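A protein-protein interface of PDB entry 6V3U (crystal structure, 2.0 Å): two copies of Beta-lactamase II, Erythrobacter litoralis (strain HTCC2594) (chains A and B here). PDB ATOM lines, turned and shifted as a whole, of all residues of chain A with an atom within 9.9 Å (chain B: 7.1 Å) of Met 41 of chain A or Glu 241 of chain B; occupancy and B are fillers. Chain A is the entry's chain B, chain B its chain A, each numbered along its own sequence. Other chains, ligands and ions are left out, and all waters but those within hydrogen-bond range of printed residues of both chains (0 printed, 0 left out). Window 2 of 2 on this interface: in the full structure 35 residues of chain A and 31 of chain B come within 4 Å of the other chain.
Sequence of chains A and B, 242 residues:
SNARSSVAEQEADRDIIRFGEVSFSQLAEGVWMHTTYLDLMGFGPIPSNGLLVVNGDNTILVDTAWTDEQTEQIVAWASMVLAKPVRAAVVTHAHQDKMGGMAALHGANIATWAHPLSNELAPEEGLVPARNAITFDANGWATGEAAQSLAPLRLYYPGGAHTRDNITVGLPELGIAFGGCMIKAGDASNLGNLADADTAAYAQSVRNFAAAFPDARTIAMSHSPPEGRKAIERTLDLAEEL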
ATOM      1  N   LEU A  38     -10.465   4.522 -30.455  1.00  0.00           N
ATOM      2  CA  LEU A  38     -10.253   4.722 -29.028  1.00  0.00           C
ATOM      3  C   LEU A  38     -10.479   3.390 -28.330  1.00  0.00           C
ATOM      4  O   LEU A  38     -11.580   2.834 -28.405  1.00  0.00           O
ATOM      5  CB  LEU A  38     -11.202   5.790 -28.478  1.00  0.00           C
ATOM      6  CG  LEU A  38     -11.139   6.012 -26.971  1.00  0.00           C
ATOM      7  CD1 LEU A  38      -9.767   6.505 -26.572  1.00  0.00           C
ATOM      8  CD2 LEU A  38     -12.204   7.003 -26.545  1.00  0.00           C
ATOM      9  N   ASP A  39      -9.436   2.878 -27.672  1.00  0.00           N
ATOM     10  CA  ASP A  39      -9.513   1.601 -26.974  1.00  0.00           C
ATOM     11  C   ASP A  39     -10.212   1.776 -25.630  1.00  0.00           C
ATOM     12  O   ASP A  39      -9.786   2.582 -24.796  1.00  0.00           O
ATOM     13  CB  ASP A  39      -8.115   1.019 -26.747  1.00  0.00           C
ATOM     14  CG  ASP A  39      -7.144   1.353 -27.863  1.00  0.00           C
ATOM     15  OD1 ASP A  39      -6.870   2.556 -28.081  1.00  0.00           O
ATOM     16  OD2 ASP A  39      -6.637   0.407 -28.507  1.00  0.00           O
ATOM     17  N   LEU A  40     -11.272   1.010 -25.412  1.00  0.00           N
ATOM     18  CA  LEU A  40     -11.978   1.016 -24.138  1.00  0.00           C
ATOM     19  C   LEU A  40     -11.922  -0.386 -23.562  1.00  0.00           C
ATOM     20  O   LEU A  40     -12.300  -1.350 -24.236  1.00  0.00           O
ATOM     21  CB  LEU A  40     -13.420   1.494 -24.313  1.00  0.00           C
ATOM     22  CG  LEU A  40     -13.460   2.954 -24.778  1.00  0.00           C
ATOM     23  CD1 LEU A  40     -14.849   3.383 -25.225  1.00  0.00           C
ATOM     24  CD2 LEU A  40     -12.941   3.871 -23.679  1.00  0.00           C
ATOM     25  N   MET A  41     -11.418  -0.496 -22.333  1.00  0.00           N
ATOM     26  CA  MET A  41     -11.303  -1.778 -21.650  1.00  0.00           C
ATOM     27  C   MET A  41     -12.639  -2.511 -21.665  1.00  0.00           C
ATOM     28  O   MET A  41     -13.639  -2.002 -21.164  1.00  0.00           O
ATOM     29  CB  MET A  41     -10.826  -1.593 -20.204  1.00  0.00           C
ATOM     30  CG  MET A  41      -9.415  -1.030 -20.040  1.00  0.00           C
ATOM     31  SD  MET A  41      -9.251   0.875 -20.457  1.00  0.00           S
ATOM     32  CE  MET A  41      -7.820   1.321 -19.203  1.00  0.00           C
ATOM     33  N   GLY A  42     -12.652  -3.697 -22.269  1.00  0.00           N
ATOM     34  CA  GLY A  42     -13.845  -4.512 -22.337  1.00  0.00           C
ATOM     35  C   GLY A  42     -14.786  -4.218 -23.489  1.00  0.00           C
ATOM     36  O   GLY A  42     -15.790  -4.927 -23.635  1.00  0.00           O
ATOM     37  N   PHE A  43     -14.501  -3.206 -24.317  1.00  0.00           N
ATOM     38  CA  PHE A  43     -15.370  -2.858 -25.434  1.00  0.00           C
ATOM     39  C   PHE A  43     -14.679  -2.869 -26.788  1.00  0.00           C
ATOM     40  O   PHE A  43     -15.364  -2.728 -27.809  1.00  0.00           O
ATOM     41  CB  PHE A  43     -16.001  -1.472 -25.220  1.00  0.00           C
ATOM     42  CG  PHE A  43     -16.962  -1.427 -24.077  1.00  0.00           C
ATOM     43  CD1 PHE A  43     -16.542  -1.029 -22.821  1.00  0.00           C
ATOM     44  CD2 PHE A  43     -18.281  -1.812 -24.249  1.00  0.00           C
ATOM     45  CE1 PHE A  43     -17.431  -1.005 -21.748  1.00  0.00           C
ATOM     46  CE2 PHE A  43     -19.179  -1.791 -23.175  1.00  0.00           C
ATOM     47  CZ  PHE A  43     -18.750  -1.386 -21.930  1.00  0.00           C
ATOM     48  N   GLY A  44     -13.360  -3.024 -26.835  1.00  0.00           N
ATOM     49  CA  GLY A  44     -12.645  -2.998 -28.086  1.00  0.00           C
ATOM     50  C   GLY A  44     -12.506  -1.588 -28.621  1.00  0.00           C
ATOM     51  O   GLY A  44     -12.952  -0.615 -27.999  1.00  0.00           O
ATOM     52  N   PRO A  45     -11.879  -1.451 -29.790  1.00  0.00           N
ATOM     53  CA  PRO A  45     -11.655  -0.115 -30.356  1.00  0.00           C
ATOM     54  C   PRO A  45     -12.951   0.503 -30.864  1.00  0.00           C
ATOM     55  O   PRO A  45     -13.790  -0.173 -31.463  1.00  0.00           O
ATOM     56  CB  PRO A  45     -10.668  -0.376 -31.506  1.00  0.00           C
ATOM     57  CG  PRO A  45     -10.087  -1.754 -31.222  1.00  0.00           C
ATOM     58  CD  PRO A  45     -11.199  -2.504 -30.563  1.00  0.00           C
ATOM     59  N   ILE A  46     -13.101   1.801 -30.630  1.00  0.00           N
ATOM     60  CA  ILE A  46     -14.331   2.528 -30.926  1.00  0.00           C
ATOM     61  C   ILE A  46     -14.031   3.562 -32.002  1.00  0.00           C
ATOM     62  O   ILE A  46     -13.214   4.470 -31.775  1.00  0.00           O
ATOM     63  CB  ILE A  46     -14.914   3.197 -29.673  1.00  0.00           C
ATOM     64  CG1 ILE A  46     -15.186   2.144 -28.590  1.00  0.00           C
ATOM     65  CG2 ILE A  46     -16.168   3.955 -30.032  1.00  0.00           C
ATOM     66  CD1 ILE A  46     -15.905   0.922 -29.104  1.00  0.00           C
ATOM     67  N   TRP A  66      -9.943  11.736 -32.055  1.00  0.00           N
ATOM     68  CA  TRP A  66     -10.003  11.620 -30.600  1.00  0.00           C
ATOM     69  C   TRP A  66      -8.937  12.481 -29.931  1.00  0.00           C
ATOM     70  O   TRP A  66      -9.218  13.203 -28.966  1.00  0.00           O
ATOM     71  CB  TRP A  66      -9.830  10.165 -30.175  1.00  0.00           C
ATOM     72  CG  TRP A  66     -10.962   9.250 -30.522  1.00  0.00           C
ATOM     73  CD1 TRP A  66     -10.980   8.322 -31.518  1.00  0.00           C
ATOM     74  CD2 TRP A  66     -12.231   9.143 -29.844  1.00  0.00           C
ATOM     75  NE1 TRP A  66     -12.178   7.649 -31.515  1.00  0.00           N
ATOM     76  CE2 TRP A  66     -12.964   8.131 -30.497  1.00  0.00           C
ATOM     77  CE3 TRP A  66     -12.813   9.806 -28.756  1.00  0.00           C
ATOM     78  CZ2 TRP A  66     -14.259   7.773 -30.110  1.00  0.00           C
ATOM     79  CZ3 TRP A  66     -14.113   9.440 -28.360  1.00  0.00           C
ATOM     80  CH2 TRP A  66     -14.814   8.436 -29.040  1.00  0.00           C
ATOM     81  N   THR A  67      -7.700  12.408 -30.420  1.00  0.00           N
ATOM     82  CA  THR A  67      -6.580  12.984 -29.702  1.00  0.00           C
ATOM     83  C   THR A  67      -5.904  14.082 -30.510  1.00  0.00           C
ATOM     84  O   THR A  67      -6.047  14.175 -31.734  1.00  0.00           O
ATOM     85  CB  THR A  67      -5.551  11.913 -29.339  1.00  0.00           C
ATOM     86  OG1 THR A  67      -4.842  11.514 -30.522  1.00  0.00           O
ATOM     87  CG2 THR A  67      -6.252  10.704 -28.714  1.00  0.00           C
ATOM     88  N   HIS A  95     -16.400  16.205 -27.889  1.00  0.00           N
ATOM     89  CA  HIS A  95     -16.254  15.261 -26.790  1.00  0.00           C
ATOM     90  C   HIS A  95     -15.687  15.997 -25.589  1.00  0.00           C
ATOM     91  O   HIS A  95     -14.699  16.727 -25.720  1.00  0.00           O
ATOM     92  CB  HIS A  95     -15.354  14.093 -27.190  1.00  0.00           C
ATOM     93  CG  HIS A  95     -15.821  13.391 -28.423  1.00  0.00           C
ATOM     94  ND1 HIS A  95     -14.962  12.956 -29.407  1.00  0.00           N
ATOM     95  CD2 HIS A  95     -17.069  13.080 -28.848  1.00  0.00           C
ATOM     96  CE1 HIS A  95     -15.658  12.392 -30.379  1.00  0.00           C
ATOM     97  NE2 HIS A  95     -16.941  12.456 -30.064  1.00  0.00           N
ATOM     98  N   GLN A  96     -16.313  15.785 -24.424  1.00  0.00           N
ATOM     99  CA  GLN A  96     -16.059  16.622 -23.253  1.00  0.00           C
ATOM    100  C   GLN A  96     -14.630  16.486 -22.749  1.00  0.00           C
ATOM    101  O   GLN A  96     -14.028  17.475 -22.318  1.00  0.00           O
ATOM    102  CB  GLN A  96     -17.031  16.262 -22.130  1.00  0.00           C
ATOM    103  CG  GLN A  96     -18.449  16.694 -22.367  1.00  0.00           C
ATOM    104  CD  GLN A  96     -19.321  16.411 -21.161  1.00  0.00           C
ATOM    105  OE1 GLN A  96     -18.924  15.680 -20.249  1.00  0.00           O
ATOM    106  NE2 GLN A  96     -20.509  16.999 -21.141  1.00  0.00           N
ATOM    107  N   ASP A  97     -14.094  15.268 -22.728  1.00  0.00           N
ATOM    108  CA  ASP A  97     -12.723  15.043 -22.284  1.00  0.00           C
ATOM    109  C   ASP A  97     -11.750  14.878 -23.438  1.00  0.00           C
ATOM    110  O   ASP A  97     -10.567  15.203 -23.290  1.00  0.00           O
ATOM    111  CB  ASP A  97     -12.643  13.798 -21.388  1.00  0.00           C
ATOM    112  CG  ASP A  97     -11.205  13.374 -21.098  1.00  0.00           C
ATOM    113  OD1 ASP A  97     -10.617  13.874 -20.115  1.00  0.00           O
ATOM    114  OD2 ASP A  97     -10.657  12.551 -21.864  1.00  0.00           O
ATOM    115  N   LYS A  98     -12.227  14.382 -24.577  1.00  0.00           N
ATOM    116  CA  LYS A  98     -11.376  14.098 -25.728  1.00  0.00           C
ATOM    117  C   LYS A  98     -11.328  15.310 -26.660  1.00  0.00           C
ATOM    118  O   LYS A  98     -11.705  15.260 -27.832  1.00  0.00           O
ATOM    119  CB  LYS A  98     -11.875  12.853 -26.451  1.00  0.00           C
ATOM    120  CG  LYS A  98     -12.215  11.690 -25.522  1.00  0.00           C
ATOM    121  CD  LYS A  98     -11.001  11.245 -24.713  1.00  0.00           C
ATOM    122  CE  LYS A  98     -10.539   9.848 -25.104  1.00  0.00           C
ATOM    123  NZ  LYS A  98      -9.150   9.832 -25.665  1.00  0.00           N
ATOM    124  N   MET A  99     -10.854  16.419 -26.104  1.00  0.00           N
ATOM    125  CA  MET A  99     -10.798  17.662 -26.850  1.00  0.00           C
ATOM    126  C   MET A  99      -9.359  18.108 -27.055  1.00  0.00           C
ATOM    127  O   MET A  99      -9.094  19.280 -27.342  1.00  0.00           O
ATOM    128  CB  MET A  99     -11.601  18.748 -26.141  1.00  0.00           C
ATOM    129  CG  MET A  99     -12.268  19.702 -27.105  1.00  0.00           C
ATOM    130  SD  MET A  99     -13.955  20.412 -26.458  1.00  0.00           S
ATOM    131  CE  MET A  99     -14.567  21.260 -28.108  1.00  0.00           C
ATOM    132  N   GLY B 186     -19.390  -5.454 -22.886  1.00  0.00           N
ATOM    133  CA  GLY B 186     -18.990  -5.767 -24.242  1.00  0.00           C
ATOM    134  C   GLY B 186     -19.778  -5.078 -25.337  1.00  0.00           C
ATOM    135  O   GLY B 186     -19.385  -5.172 -26.507  1.00  0.00           O
ATOM    136  N   THR B 199     -21.787  13.760 -21.161  1.00  0.00           N
ATOM    137  CA  THR B 199     -21.232  12.632 -20.424  1.00  0.00           C
ATOM    138  C   THR B 199     -21.109  12.957 -18.941  1.00  0.00           C
ATOM    139  O   THR B 199     -21.440  12.124 -18.089  1.00  0.00           O
ATOM    140  CB  THR B 199     -19.872  12.243 -21.018  1.00  0.00           C
ATOM    141  OG1 THR B 199     -19.932  12.307 -22.452  1.00  0.00           O
ATOM    142  CG2 THR B 199     -19.505  10.828 -20.621  1.00  0.00           C
ATOM    143  N   ARG B 234     -19.132  -0.129 -14.454  1.00  0.00           N
ATOM    144  CA  ARG B 234     -18.800  -0.158 -15.872  1.00  0.00           C
ATOM    145  C   ARG B 234     -19.233   1.129 -16.560  1.00  0.00           C
ATOM    146  O   ARG B 234     -18.485   1.695 -17.367  1.00  0.00           O
ATOM    147  CB  ARG B 234     -19.458  -1.362 -16.543  1.00  0.00           C
ATOM    148  CG  ARG B 234     -19.424  -1.274 -18.054  1.00  0.00           C
ATOM    149  CD  ARG B 234     -19.746  -2.594 -18.701  1.00  0.00           C
ATOM    150  NE  ARG B 234     -21.077  -3.048 -18.340  1.00  0.00           N
ATOM    151  CZ  ARG B 234     -21.331  -4.125 -17.600  1.00  0.00           C
ATOM    152  NH1 ARG B 234     -22.588  -4.462 -17.311  1.00  0.00           N
ATOM    153  NH2 ARG B 234     -20.326  -4.875 -17.170  1.00  0.00           N
ATOM    154  N   LEU B 236     -19.676   4.061 -15.128  1.00  0.00           N
ATOM    155  CA  LEU B 236     -18.867   5.176 -14.638  1.00  0.00           C
ATOM    156  C   LEU B 236     -17.445   5.135 -15.182  1.00  0.00           C
ATOM    157  O   LEU B 236     -16.798   6.182 -15.282  1.00  0.00           O
ATOM    158  CB  LEU B 236     -18.813   5.194 -13.114  1.00  0.00           C
ATOM    159  CG  LEU B 236     -20.046   5.628 -12.319  1.00  0.00           C
ATOM    160  CD1 LEU B 236     -19.754   5.515 -10.823  1.00  0.00           C
ATOM    161  CD2 LEU B 236     -20.449   7.045 -12.687  1.00  0.00           C
ATOM    162  N   ASP B 237     -16.927   3.941 -15.484  1.00  0.00           N
ATOM    163  CA  ASP B 237     -15.605   3.851 -16.097  1.00  0.00           C
ATOM    164  C   ASP B 237     -15.601   4.497 -17.478  1.00  0.00           C
ATOM    165  O   ASP B 237     -14.693   5.266 -17.807  1.00  0.00           O
ATOM    166  CB  ASP B 237     -15.159   2.389 -16.189  1.00  0.00           C
ATOM    167  CG  ASP B 237     -14.947   1.754 -14.826  1.00  0.00           C
ATOM    168  OD1 ASP B 237     -14.603   2.488 -13.874  1.00  0.00           O
ATOM    169  OD2 ASP B 237     -15.132   0.521 -14.701  1.00  0.00           O
ATOM    170  N   LEU B 238     -16.625   4.209 -18.286  1.00  0.00           N
ATOM    171  CA  LEU B 238     -16.724   4.799 -19.615  1.00  0.00           C
ATOM    172  C   LEU B 238     -16.798   6.320 -19.549  1.00  0.00           C
ATOM    173  O   LEU B 238     -16.079   7.014 -20.280  1.00  0.00           O
ATOM    174  CB  LEU B 238     -17.939   4.228 -20.345  1.00  0.00           C
ATOM    175  CG  LEU B 238     -17.853   2.739 -20.690  1.00  0.00           C
ATOM    176  CD1 LEU B 238     -19.222   2.196 -21.079  1.00  0.00           C
ATOM    177  CD2 LEU B 238     -16.845   2.489 -21.798  1.00  0.00           C
ATOM    178  N   ALA B 239     -17.641   6.854 -18.661  1.00  0.00           N
ATOM    179  CA  ALA B 239     -17.868   8.295 -18.614  1.00  0.00           C
ATOM    180  C   ALA B 239     -16.595   9.078 -18.315  1.00  0.00           C
ATOM    181  O   ALA B 239     -16.467  10.228 -18.753  1.00  0.00           O
ATOM    182  CB  ALA B 239     -18.944   8.623 -17.582  1.00  0.00           C
ATOM    183  N   GLU B 240     -15.644   8.494 -17.582  1.00  0.00           N
ATOM    184  CA  GLU B 240     -14.385   9.201 -17.368  1.00  0.00           C
ATOM    185  C   GLU B 240     -13.495   9.131 -18.605  1.00  0.00           C
ATOM    186  O   GLU B 240     -12.838  10.119 -18.961  1.00  0.00           O
ATOM    187  CB  GLU B 240     -13.658   8.636 -16.143  1.00  0.00           C
ATOM    188  CG  GLU B 240     -12.663   9.603 -15.490  1.00  0.00           C
ATOM    189  CD  GLU B 240     -11.408   9.857 -16.330  1.00  0.00           C
ATOM    190  OE1 GLU B 240     -10.987   8.949 -17.080  1.00  0.00           O
ATOM    191  OE2 GLU B 240     -10.843  10.967 -16.242  1.00  0.00           O
ATOM    192  N   GLU B 241     -13.458   7.975 -19.272  1.00  0.00           N
ATOM    193  CA  GLU B 241     -12.679   7.829 -20.498  1.00  0.00           C
ATOM    194  C   GLU B 241     -13.319   8.538 -21.686  1.00  0.00           C
ATOM    195  O   GLU B 241     -12.711   8.586 -22.758  1.00  0.00           O
ATOM    196  CB  GLU B 241     -12.482   6.341 -20.810  1.00  0.00           C
ATOM    197  CG  GLU B 241     -12.035   5.519 -19.596  1.00  0.00           C
ATOM    198  CD  GLU B 241     -12.194   4.013 -19.782  1.00  0.00           C
ATOM    199  OE1 GLU B 241     -11.183   3.289 -19.694  1.00  0.00           O
ATOM    200  OE2 GLU B 241     -13.331   3.548 -20.011  1.00  0.00           O
ATOM    201  N   LEU B 242     -14.523   9.082 -21.524  1.00  0.00           N
ATOM    202  CA  LEU B 242     -15.172   9.871 -22.562  1.00  0.00           C
ATOM    203  C   LEU B 242     -15.510  11.269 -22.044  1.00  0.00           C
ATOM    204  O   LEU B 242     -16.325  11.985 -22.635  1.00  0.00           O
ATOM    205  CB  LEU B 242     -16.440   9.174 -23.052  1.00  0.00           C
ATOM    206  CG  LEU B 242     -16.255   7.748 -23.571  1.00  0.00           C
ATOM    207  CD1 LEU B 242     -17.612   7.038 -23.678  1.00  0.00           C
ATOM    208  CD2 LEU B 242     -15.517   7.765 -24.901  1.00  0.00           C
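Among the printed residues, merely in contact across the chains: Gly 42 of chain A with Gly 186 of chain B, Lys 98 of chain A with Glu 241 of chain B, Phe 43 of chain A with Leu 238 of chain B, Phe 43 of chain A with Arg 234 of chain B, Phe 43 of chain A with Gly 186 of chain B, Leu 40 of chain A with Glu 241 of chain B, Leu 38 of chain A with Leu 242 of chain B and Asp 97 of chain A with Leu 242 of chain B.
The backbone carbonyl oxygen of Leu 38 of chain A sits at hydrogen-bond distance from the backbone NH of Ile 46 of chain A (2.9 Å).
Of the printed residues of chain B, Leu 38 of chain A touches Leu 242. Of the printed residues of chain B, Leu 40 of chain A touches Glu 241 (3.7 Å). Ile 46 of chain A touches none of the printed residues of chain B. Of the printed residues of chain B, Gln 96 of chain A touches Thr 199 (3.5 Å). Met 99 of chain A touches none of the printed residues of chain B. No residue of chain A comes within 4 Å of Ala 239 of chain B. No residue of chain A comes within 4 Å of Glu 240 of chain B. The nearest residue of chain A that does not touch Glu 241 of chain B is Leu 38 of chain A (4.1 Å).
N of Thr 199 of chain B lies close to NE2 of Gln 96 of chain A (3.5 Å). The side-chain carboxylate (OE1) of Glu 241 of chain B lies close to the side-chain sulfur (SD) of Met 41 of chain A (3.2 Å).
Of the 10 printed residues of chain B, 6 touch a printed residue of chain A. Printed residues of chain B that touch a printed residue of chain A: Gly 186, Thr 199, Arg 234, Leu 238, Glu 241 and Leu 242. Hydrophobic or aromatic side chains of chain B that line the printed part of chain A: Leu 238 and Leu 242. Hydrophobic or aromatic side chains of chain A within 4 Å of the printed part of chain B: Leu 38, Leu 40, Met 41 and Phe 43. Among the printed residues, no Asp or Glu carboxylate lies within 4 Å of a Lys or Arg side-chain nitrogen of the other chain.
No position is printed for both chains. Of the 10 pairs that touch across the chains among the printed residues, none has its exchanged pair printed and touching as well.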
